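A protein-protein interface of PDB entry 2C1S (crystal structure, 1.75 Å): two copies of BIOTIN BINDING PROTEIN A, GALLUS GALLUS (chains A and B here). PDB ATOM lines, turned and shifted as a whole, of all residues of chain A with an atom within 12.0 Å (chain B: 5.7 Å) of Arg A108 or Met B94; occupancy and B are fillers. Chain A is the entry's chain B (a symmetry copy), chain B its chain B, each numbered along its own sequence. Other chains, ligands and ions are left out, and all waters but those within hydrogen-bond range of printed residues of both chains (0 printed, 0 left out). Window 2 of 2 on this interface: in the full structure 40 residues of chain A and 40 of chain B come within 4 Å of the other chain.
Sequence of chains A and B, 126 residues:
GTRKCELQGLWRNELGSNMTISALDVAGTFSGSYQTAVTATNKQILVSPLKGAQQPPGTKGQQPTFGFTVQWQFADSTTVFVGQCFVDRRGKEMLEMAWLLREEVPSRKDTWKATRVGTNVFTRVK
OE1 of Gln B84 lies within hydrogen-bond range of NH1 of Arg A102 (2.5 Å). The backbone NH (N) of Val A105 sits at hydrogen-bond distance from the side-chain amide oxygen (OE1) of Gln B84 (2.9 Å). The side-chain carboxylate (OE2) of Glu B96 is in salt-bridge range of the guanidinium group (NE) of Arg A108 (2.6 Å).
N of Phe B86 sits at hydrogen-bond distance from SG of Cys B5 (3.6 Å). The backbone NH (N) of Phe B86 is in hydrogen-bond range of the backbone carbonyl oxygen (O) of Met B94, at 2.8 Å. The backbone carbonyl oxygen (O) of Ala A114 is in hydrogen-bond range of the backbone NH (N) of Glu A103 (2.9 Å). N of Lys A109 lies close to OG of Ser A107 (3.5 Å). O of Arg A108 is in hydrogen-bond range of OG1 of Thr A111, 2.5 Å away. The side-chain sulfur (SG) of Cys B5 forms a disulfide with the side-chain sulfur (SG) of Cys B85, 2.1 Å away.
Among the printed residues, merely in contact across the chains: Thr A111 with Glu B96, Glu A104 with Gln B84, Thr A111 with Phe B86, Arg A108 with Phe B86, Ser A107 with Phe B86, Arg A108 with Val B121, Glu A103 with Gln B84, Arg A102 with Phe B86, Val A105 with Phe B86 and Arg A108 with Met B94.
Of the printed residues of chain B, Glu A104 touches Gln B84 (3.4 Å). Of the printed residues of chain B, Val A105 touches Gln B84 and Phe B86. Of the printed residues of chain B, Thr A111 touches Phe B86 and Glu B96. Trp A112 touches none of the printed residues of chain B. No residue of chain A comes within 4 Å of Cys B5. Trp B11 touches none of the printed residues of chain A. No residue of chain A comes within 4 Å of Cys B85. Of the printed residues of chain A, Phe B86 touches Arg A102 (3.7 Å), Val A105 (3.7 Å), Ser A107 (3.5 Å), Arg A108 (3.5 Å) and Thr A111 (3.5 Å). No residue of chain A comes within 4 Å of Val B87. No residue of chain A comes within 4 Å of Asp B88. No residue of chain A comes within 4 Å of Lys B92. Glu B93 touches none of the printed residues of chain A. No residue of chain A comes within 4 Å of Leu B95. Of chain A, only Arg A108 (3.6 Å) comes within 4 Å of Val B121. The nearest printed residue of chain A that does not touch Met B94 is Thr A111 (7.7 Å).
Of the 14 printed residues of chain A, 7 touch a printed residue of chain B. Printed residues of chain A that touch a printed residue of chain B: Arg A102, Glu A103, Glu A104, Val A105, Ser A107, Arg A108 and Thr A111. Of the 15 printed residues of chain B, 5 touch a printed residue of chain A. Hydrophobic or aromatic side chains of chain B within 4 Å of the printed part of chain A: Phe B86, Met B94 and Val B121. Among the printed residues, Asp or Glu carboxylates within 4 Å of a Lys or Arg side-chain nitrogen of the other chain: Arg A108 with Glu B96.
No position is printed for both chains. Of the 13 pairs that touch across the chains among the printed residues, none has its exchanged pair printed and touching as well.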
ATOM      1  N   ARG A 102      13.244  25.735 -31.422  1.00  0.00           N
ATOM      2  CA  ARG A 102      13.534  24.300 -31.502  1.00  0.00           C
ATOM      3  C   ARG A 102      13.498  23.870 -32.945  1.00  0.00           C
ATOM      4  O   ARG A 102      12.467  24.044 -33.627  1.00  0.00           O
ATOM      5  CB  ARG A 102      12.477  23.505 -30.740  1.00  0.00           C
ATOM      6  CG  ARG A 102      12.637  21.957 -30.717  1.00  0.00           C
ATOM      7  CD  ARG A 102      14.029  21.500 -30.343  1.00  0.00           C
ATOM      8  NE  ARG A 102      14.227  20.077 -29.959  1.00  0.00           N
ATOM      9  CZ  ARG A 102      14.263  19.030 -30.787  1.00  0.00           C
ATOM     10  NH1 ARG A 102      14.057  19.180 -32.076  1.00  0.00           N
ATOM     11  NH2 ARG A 102      14.522  17.813 -30.311  1.00  0.00           N
ATOM     12  N   GLU A 103      14.596  23.289 -33.406  1.00  0.00           N
ATOM     13  CA  GLU A 103      14.627  22.677 -34.755  1.00  0.00           C
ATOM     14  C   GLU A 103      14.268  21.184 -34.738  1.00  0.00           C
ATOM     15  O   GLU A 103      14.453  20.504 -33.747  1.00  0.00           O
ATOM     16  CB  GLU A 103      15.983  22.947 -35.392  1.00  0.00           C
ATOM     17  CG  GLU A 103      15.967  24.353 -36.004  1.00  0.00           C
ATOM     18  CD  GLU A 103      17.322  24.994 -36.195  1.00  0.00           C
ATOM     19  OE1 GLU A 103      18.349  24.292 -36.451  1.00  0.00           O
ATOM     20  OE2 GLU A 103      17.341  26.254 -36.095  1.00  0.00           O
ATOM     21  N   GLU A 104      13.686  20.711 -35.834  1.00  0.00           N
ATOM     22  CA  GLU A 104      13.333  19.321 -35.962  1.00  0.00           C
ATOM     23  C   GLU A 104      14.624  18.636 -36.371  1.00  0.00           C
ATOM     24  O   GLU A 104      15.243  19.008 -37.379  1.00  0.00           O
ATOM     25  CB  GLU A 104      12.240  19.165 -37.020  1.00  0.00           C
ATOM     26  CG  GLU A 104      11.726  17.757 -37.174  1.00  0.00           C
ATOM     27  CD  GLU A 104      10.964  17.591 -38.480  1.00  0.00           C
ATOM     28  OE1 GLU A 104       9.836  18.137 -38.617  1.00  0.00           O
ATOM     29  OE2 GLU A 104      11.533  16.941 -39.377  1.00  0.00           O
ATOM     30  N   VAL A 105      15.083  17.702 -35.553  1.00  0.00           N
ATOM     31  CA  VAL A 105      16.340  17.009 -35.869  1.00  0.00           C
ATOM     32  C   VAL A 105      16.077  15.584 -36.358  1.00  0.00           C
ATOM     33  O   VAL A 105      15.034  14.995 -36.034  1.00  0.00           O
ATOM     34  CB  VAL A 105      17.368  17.043 -34.690  1.00  0.00           C
ATOM     35  CG1 VAL A 105      17.860  18.493 -34.430  1.00  0.00           C
ATOM     36  CG2 VAL A 105      16.814  16.406 -33.425  1.00  0.00           C
ATOM     37  N   PRO A 106      17.014  15.031 -37.157  1.00  0.00           N
ATOM     38  CA  PRO A 106      16.899  13.690 -37.741  1.00  0.00           C
ATOM     39  C   PRO A 106      16.915  12.544 -36.746  1.00  0.00           C
ATOM     40  O   PRO A 106      16.333  11.481 -37.025  1.00  0.00           O
ATOM     41  CB  PRO A 106      18.158  13.589 -38.626  1.00  0.00           C
ATOM     42  CG  PRO A 106      18.559  14.974 -38.901  1.00  0.00           C
ATOM     43  CD  PRO A 106      18.260  15.684 -37.596  1.00  0.00           C
ATOM     44  N   SER A 107      17.608  12.697 -35.625  1.00  0.00           N
ATOM     45  CA  SER A 107      17.667  11.604 -34.654  1.00  0.00           C
ATOM     46  C   SER A 107      17.766  12.104 -33.229  1.00  0.00           C
ATOM     47  O   SER A 107      18.084  13.272 -33.010  1.00  0.00           O
ATOM     48  CB  SER A 107      18.809  10.615 -34.964  1.00  0.00           C
ATOM     49  OG  SER A 107      20.079  11.107 -34.612  1.00  0.00           O
ATOM     50  N   ARG A 108      17.472  11.219 -32.280  1.00  0.00           N
ATOM     51  CA  ARG A 108      17.482  11.593 -30.877  1.00  0.00           C
ATOM     52  C   ARG A 108      18.884  12.036 -30.483  1.00  0.00           C
ATOM     53  O   ARG A 108      19.034  12.929 -29.645  1.00  0.00           O
ATOM     54  CB  ARG A 108      16.981  10.475 -29.971  1.00  0.00           C
ATOM     55  CG  ARG A 108      16.677  10.955 -28.564  1.00  0.00           C
ATOM     56  CD  ARG A 108      16.161   9.862 -27.637  1.00  0.00           C
ATOM     57  NE  ARG A 108      16.046  10.388 -26.275  1.00  0.00           N
ATOM     58  CZ  ARG A 108      15.893   9.663 -25.172  1.00  0.00           C
ATOM     59  NH1 ARG A 108      15.824   8.337 -25.229  1.00  0.00           N
ATOM     60  NH2 ARG A 108      15.824  10.275 -24.003  1.00  0.00           N
ATOM     61  N   LYS A 109      19.895  11.458 -31.137  1.00  0.00           N
ATOM     62  CA  LYS A 109      21.297  11.758 -30.843  1.00  0.00           C
ATOM     63  C   LYS A 109      21.683  13.195 -31.209  1.00  0.00           C
ATOM     64  O   LYS A 109      22.698  13.706 -30.741  1.00  0.00           O
ATOM     65  CB  LYS A 109      22.233  10.760 -31.540  1.00  0.00           C
ATOM     66  CG  LYS A 109      22.080   9.350 -31.033  1.00  0.00           C
ATOM     67  CD  LYS A 109      23.169   8.423 -31.568  1.00  0.00           C
ATOM     68  CE  LYS A 109      23.023   7.020 -30.965  1.00  0.00           C
ATOM     69  NZ  LYS A 109      23.028   6.994 -29.458  1.00  0.00           N
ATOM     70  N   ASP A 110      20.860  13.840 -32.029  1.00  0.00           N
ATOM     71  CA  ASP A 110      21.088  15.231 -32.393  1.00  0.00           C
ATOM     72  C   ASP A 110      20.291  16.192 -31.504  1.00  0.00           C
ATOM     73  O   ASP A 110      20.346  17.405 -31.724  1.00  0.00           O
ATOM     74  CB  ASP A 110      20.666  15.493 -33.834  1.00  0.00           C
ATOM     75  CG  ASP A 110      21.476  14.712 -34.825  1.00  0.00           C
ATOM     76  OD1 ASP A 110      22.626  14.366 -34.493  1.00  0.00           O
ATOM     77  OD2 ASP A 110      20.936  14.438 -35.915  1.00  0.00           O
ATOM     78  N   THR A 111      19.545  15.673 -30.534  1.00  0.00           N
ATOM     79  CA  THR A 111      18.678  16.592 -29.726  1.00  0.00           C
ATOM     80  C   THR A 111      19.470  17.646 -28.993  1.00  0.00           C
ATOM     81  O   THR A 111      18.968  18.775 -28.817  1.00  0.00           O
ATOM     82  CB  THR A 111      17.750  15.821 -28.731  1.00  0.00           C
ATOM     83  OG1 THR A 111      17.250  14.634 -29.343  1.00  0.00           O
ATOM     84  CG2 THR A 111      16.557  16.672 -28.363  1.00  0.00           C
ATOM     85  N   TRP A 112      20.702  17.307 -28.576  1.00  0.00           N
ATOM     86  CA  TRP A 112      21.526  18.255 -27.795  1.00  0.00           C
ATOM     87  C   TRP A 112      21.691  19.603 -28.534  1.00  0.00           C
ATOM     88  O   TRP A 112      21.814  20.622 -27.863  1.00  0.00           O
ATOM     89  CB  TRP A 112      22.912  17.686 -27.471  1.00  0.00           C
ATOM     90  CG  TRP A 112      23.753  17.543 -28.709  1.00  0.00           C
ATOM     91  CD1 TRP A 112      23.785  16.476 -29.576  1.00  0.00           C
ATOM     92  CD2 TRP A 112      24.629  18.517 -29.239  1.00  0.00           C
ATOM     93  NE1 TRP A 112      24.657  16.728 -30.608  1.00  0.00           N
ATOM     94  CE2 TRP A 112      25.188  17.982 -30.429  1.00  0.00           C
ATOM     95  CE3 TRP A 112      25.020  19.798 -28.819  1.00  0.00           C
ATOM     96  CZ2 TRP A 112      26.113  18.687 -31.204  1.00  0.00           C
ATOM     97  CZ3 TRP A 112      25.923  20.504 -29.604  1.00  0.00           C
ATOM     98  CH2 TRP A 112      26.489  19.934 -30.764  1.00  0.00           C
ATOM     99  N   LYS A 113      21.673  19.596 -29.873  1.00  0.00           N
ATOM    100  CA  LYS A 113      21.976  20.786 -30.679  1.00  0.00           C
ATOM    101  C   LYS A 113      20.710  21.503 -31.202  1.00  0.00           C
ATOM    102  O   LYS A 113      20.796  22.472 -31.970  1.00  0.00           O
ATOM    103  CB  LYS A 113      22.941  20.469 -31.831  1.00  0.00           C
ATOM    104  CG  LYS A 113      22.368  19.554 -32.926  1.00  0.00           C
ATOM    105  CD  LYS A 113      23.447  19.250 -33.973  1.00  0.00           C
ATOM    106  CE  LYS A 113      22.866  18.422 -35.115  1.00  0.00           C
ATOM    107  NZ  LYS A 113      23.868  18.208 -36.186  1.00  0.00           N
ATOM    108  N   ALA A 114      19.550  21.060 -30.747  1.00  0.00           N
ATOM    109  CA  ALA A 114      18.313  21.434 -31.425  1.00  0.00           C
ATOM    110  C   ALA A 114      17.719  22.786 -30.950  1.00  0.00           C
ATOM    111  O   ALA A 114      16.801  23.288 -31.571  1.00  0.00           O
ATOM    112  CB  ALA A 114      17.280  20.325 -31.287  1.00  0.00           C
ATOM    113  N   THR A 115      18.236  23.369 -29.875  1.00  0.00           N
ATOM    114  CA  THR A 115      17.509  24.481 -29.234  1.00  0.00           C
ATOM    115  C   THR A 115      18.380  25.700 -29.073  1.00  0.00           C
ATOM    116  O   THR A 115      19.397  25.636 -28.400  1.00  0.00           O
ATOM    117  CB  THR A 115      17.066  24.095 -27.814  1.00  0.00           C
ATOM    118  OG1 THR A 115      16.386  22.833 -27.848  1.00  0.00           O
ATOM    119  CG2 THR A 115      16.109  25.153 -27.251  1.00  0.00           C
ATOM    120  N   CYS B   5       4.326   8.289 -31.036  1.00  0.00           N
ATOM    121  CA  CYS B   5       4.697   9.681 -30.776  1.00  0.00           C
ATOM    122  C   CYS B   5       3.562  10.683 -30.945  1.00  0.00           C
ATOM    123  O   CYS B   5       3.811  11.906 -30.963  1.00  0.00           O
ATOM    124  CB  CYS B   5       5.925  10.089 -31.590  1.00  0.00           C
ATOM    125  SG  CYS B   5       7.486   9.870 -30.717  1.00  0.00           S
ATOM    126  N   TRP B  11       1.814  11.602 -20.040  1.00  0.00           N
ATOM    127  CA  TRP B  11       3.290  11.607 -20.073  1.00  0.00           C
ATOM    128  C   TRP B  11       3.864  11.896 -18.695  1.00  0.00           C
ATOM    129  O   TRP B  11       3.206  12.483 -17.854  1.00  0.00           O
ATOM    130  CB  TRP B  11       3.830  12.650 -21.071  1.00  0.00           C
ATOM    131  CG  TRP B  11       3.368  12.447 -22.481  1.00  0.00           C
ATOM    132  CD1 TRP B  11       2.215  12.920 -23.026  1.00  0.00           C
ATOM    133  CD2 TRP B  11       4.035  11.717 -23.529  1.00  0.00           C
ATOM    134  NE1 TRP B  11       2.127  12.539 -24.347  1.00  0.00           N
ATOM    135  CE2 TRP B  11       3.222  11.801 -24.682  1.00  0.00           C
ATOM    136  CE3 TRP B  11       5.245  11.019 -23.614  1.00  0.00           C
ATOM    137  CZ2 TRP B  11       3.576  11.197 -25.901  1.00  0.00           C
ATOM    138  CZ3 TRP B  11       5.594  10.422 -24.816  1.00  0.00           C
ATOM    139  CH2 TRP B  11       4.776  10.523 -25.946  1.00  0.00           C
ATOM    140  N   GLN B  84      10.415  17.823 -29.219  1.00  0.00           N
ATOM    141  CA  GLN B  84      10.235  16.902 -30.316  1.00  0.00           C
ATOM    142  C   GLN B  84      10.196  15.502 -29.708  1.00  0.00           C
ATOM    143  O   GLN B  84      10.987  15.198 -28.814  1.00  0.00           O
ATOM    144  CB  GLN B  84      11.405  17.031 -31.279  1.00  0.00           C
ATOM    145  CG  GLN B  84      11.283  16.112 -32.518  1.00  0.00           C
ATOM    146  CD  GLN B  84      12.418  16.303 -33.507  1.00  0.00           C
ATOM    147  OE1 GLN B  84      13.354  17.066 -33.278  1.00  0.00           O
ATOM    148  NE2 GLN B  84      12.349  15.565 -34.621  1.00  0.00           N
ATOM    149  N   CYS B  85       9.279  14.665 -30.194  1.00  0.00           N
ATOM    150  CA  CYS B  85       9.194  13.277 -29.754  1.00  0.00           C
ATOM    151  C   CYS B  85      10.158  12.398 -30.554  1.00  0.00           C
ATOM    152  O   CYS B  85      10.434  12.666 -31.723  1.00  0.00           O
ATOM    153  CB  CYS B  85       7.751  12.768 -29.894  1.00  0.00           C
ATOM    154  SG  CYS B  85       7.381  11.167 -29.109  1.00  0.00           S
ATOM    155  N   PHE B  86      10.689  11.374 -29.895  1.00  0.00           N
ATOM    156  CA  PHE B  86      11.510  10.341 -30.562  1.00  0.00           C
ATOM    157  C   PHE B  86      10.988   8.972 -30.190  1.00  0.00           C
ATOM    158  O   PHE B  86      10.494   8.767 -29.090  1.00  0.00           O
ATOM    159  CB  PHE B  86      12.995  10.493 -30.219  1.00  0.00           C
ATOM    160  CG  PHE B  86      13.552  11.824 -30.628  1.00  0.00           C
ATOM    161  CD1 PHE B  86      14.119  12.004 -31.896  1.00  0.00           C
ATOM    162  CD2 PHE B  86      13.452  12.917 -29.778  1.00  0.00           C
ATOM    163  CE1 PHE B  86      14.608  13.249 -32.304  1.00  0.00           C
ATOM    164  CE2 PHE B  86      13.924  14.157 -30.172  1.00  0.00           C
ATOM    165  CZ  PHE B  86      14.509  14.328 -31.440  1.00  0.00           C
ATOM    166  N   VAL B  87      11.067   8.043 -31.135  1.00  0.00           N
ATOM    167  CA  VAL B  87      10.657   6.665 -30.881  1.00  0.00           C
ATOM    168  C   VAL B  87      11.909   5.801 -31.076  1.00  0.00           C
ATOM    169  O   VAL B  87      12.571   5.907 -32.106  1.00  0.00           O
ATOM    170  CB  VAL B  87       9.426   6.249 -31.780  1.00  0.00           C
ATOM    171  CG1 VAL B  87       9.558   6.805 -33.198  1.00  0.00           C
ATOM    172  CG2 VAL B  87       9.219   4.721 -31.791  1.00  0.00           C
ATOM    173  N   ASP B  88      12.274   5.026 -30.050  1.00  0.00           N
ATOM    174  CA  ASP B  88      13.475   4.184 -30.118  1.00  0.00           C
ATOM    175  C   ASP B  88      13.198   2.872 -30.862  1.00  0.00           C
ATOM    176  O   ASP B  88      12.075   2.652 -31.345  1.00  0.00           O
ATOM    177  CB  ASP B  88      14.106   3.949 -28.724  1.00  0.00           C
ATOM    178  CG  ASP B  88      13.336   2.952 -27.862  1.00  0.00           C
ATOM    179  OD1 ASP B  88      12.336   2.355 -28.306  1.00  0.00           O
ATOM    180  OD2 ASP B  88      13.741   2.764 -26.700  1.00  0.00           O
ATOM    181  N   LYS B  92       9.471   2.681 -27.651  1.00  0.00           N
ATOM    182  CA  LYS B  92       9.329   3.553 -26.498  1.00  0.00           C
ATOM    183  C   LYS B  92       9.440   5.005 -26.973  1.00  0.00           C
ATOM    184  O   LYS B  92      10.411   5.372 -27.644  1.00  0.00           O
ATOM    185  CB  LYS B  92      10.391   3.244 -25.448  1.00  0.00           C
ATOM    186  CG  LYS B  92      10.091   3.914 -24.126  1.00  0.00           C
ATOM    187  CD  LYS B  92      10.957   3.424 -22.993  1.00  0.00           C
ATOM    188  CE  LYS B  92      10.333   3.798 -21.667  1.00  0.00           C
ATOM    189  NZ  LYS B  92      11.311   3.594 -20.563  1.00  0.00           N
ATOM    190  N   GLU B  93       8.430   5.807 -26.640  1.00  0.00           N
ATOM    191  CA  GLU B  93       8.368   7.217 -27.035  1.00  0.00           C
ATOM    192  C   GLU B  93       8.983   8.074 -25.955  1.00  0.00           C
ATOM    193  O   GLU B  93       8.796   7.831 -24.758  1.00  0.00           O
ATOM    194  CB  GLU B  93       6.918   7.667 -27.226  1.00  0.00           C
ATOM    195  CG  GLU B  93       6.192   6.947 -28.362  1.00  0.00           C
ATOM    196  CD  GLU B  93       4.748   6.658 -28.022  1.00  0.00           C
ATOM    197  OE1 GLU B  93       4.462   6.122 -26.924  1.00  0.00           O
ATOM    198  OE2 GLU B  93       3.903   6.974 -28.856  1.00  0.00           O
ATOM    199  N   MET B  94       9.704   9.099 -26.383  1.00  0.00           N
ATOM    200  CA  MET B  94      10.247  10.071 -25.437  1.00  0.00           C
ATOM    201  C   MET B  94      10.086  11.457 -26.017  1.00  0.00           C
ATOM    202  O   MET B  94      10.459  11.695 -27.165  1.00  0.00           O
ATOM    203  CB  MET B  94      11.733   9.821 -25.164  1.00  0.00           C
ATOM    204  CG  MET B  94      12.005   8.665 -24.206  1.00  0.00           C
ATOM    205  SD  MET B  94      12.035   7.081 -25.068  1.00  0.00           S
ATOM    206  CE  MET B  94      12.995   6.088 -23.905  1.00  0.00           C
ATOM    207  N   LEU B  95       9.549  12.373 -25.216  1.00  0.00           N
ATOM    208  CA  LEU B  95       9.531  13.784 -25.628  1.00  0.00           C
ATOM    209  C   LEU B  95      10.784  14.450 -25.043  1.00  0.00           C
ATOM    210  O   LEU B  95      10.962  14.455 -23.815  1.00  0.00           O
ATOM    211  CB  LEU B  95       8.280  14.489 -25.090  1.00  0.00           C
ATOM    212  CG  LEU B  95       6.885  13.891 -25.302  1.00  0.00           C
ATOM    213  CD1 LEU B  95       5.864  14.795 -24.627  1.00  0.00           C
ATOM    214  CD2 LEU B  95       6.581  13.767 -26.780  1.00  0.00           C
ATOM    215  N   GLU B  96      11.666  14.944 -25.924  1.00  0.00           N
ATOM    216  CA  GLU B  96      12.829  15.720 -25.509  1.00  0.00           C
ATOM    217  C   GLU B  96      12.431  17.186 -25.498  1.00  0.00           C
ATOM    218  O   GLU B  96      12.030  17.709 -26.549  1.00  0.00           O
ATOM    219  CB  GLU B  96      13.963  15.514 -26.498  1.00  0.00           C
ATOM    220  CG  GLU B  96      14.587  14.115 -26.466  1.00  0.00           C
ATOM    221  CD  GLU B  96      15.476  13.840 -25.251  1.00  0.00           C
ATOM    222  OE1 GLU B  96      15.768  14.753 -24.453  1.00  0.00           O
ATOM    223  OE2 GLU B  96      15.917  12.665 -25.108  1.00  0.00           O
ATOM    224  N   VAL B 121      12.826  15.182 -20.016  1.00  0.00           N
ATOM    225  CA  VAL B 121      12.522  14.090 -20.943  1.00  0.00           C
ATOM    226  C   VAL B 121      11.271  13.422 -20.430  1.00  0.00           C
ATOM    227  O   VAL B 121      11.246  12.990 -19.272  1.00  0.00           O
ATOM    228  CB  VAL B 121      13.629  12.988 -21.002  1.00  0.00           C
ATOM    229  CG1 VAL B 121      13.268  11.983 -22.115  1.00  0.00           C
ATOM    230  CG2 VAL B 121      14.987  13.598 -21.236  1.00  0.00           C
ATOM    231  N   PHE B 122      10.256  13.308 -21.287  1.00  0.00           N
ATOM    232  CA  PHE B 122       8.987  12.693 -20.897  1.00  0.00           C
ATOM    233  C   PHE B 122       8.886  11.335 -21.534  1.00  0.00           C
ATOM    234  O   PHE B 122       9.226  11.175 -22.705  1.00  0.00           O
ATOM    235  CB  PHE B 122       7.792  13.498 -21.415  1.00  0.00           C
ATOM    236  CG  PHE B 122       7.638  14.834 -20.756  1.00  0.00           C
ATOM    237  CD1 PHE B 122       6.727  15.016 -19.721  1.00  0.00           C
ATOM    238  CD2 PHE B 122       8.430  15.904 -21.180  1.00  0.00           C
ATOM    239  CE1 PHE B 122       6.598  16.235 -19.089  1.00  0.00           C
ATOM    240  CE2 PHE B 122       8.280  17.160 -20.601  1.00  0.00           C
ATOM    241  CZ  PHE B 122       7.371  17.326 -19.553  1.00  0.00           C
ATOM    242  N   THR B 123       8.379  10.371 -20.770  1.00  0.00           N
ATOM    243  CA  THR B 123       8.014   9.083 -21.341  1.00  0.00           C
ATOM    244  C   THR B 123       6.498   8.891 -21.201  1.00  0.00           C
ATOM    245  O   THR B 123       5.859   9.456 -20.298  1.00  0.00           O
ATOM    246  CB  THR B 123       8.732   7.917 -20.610  1.00  0.00           C
ATOM    247  OG1 THR B 123       8.382   7.964 -19.219  1.00  0.00           O
ATOM    248  CG2 THR B 123      10.219   8.025 -20.756  1.00  0.00           C
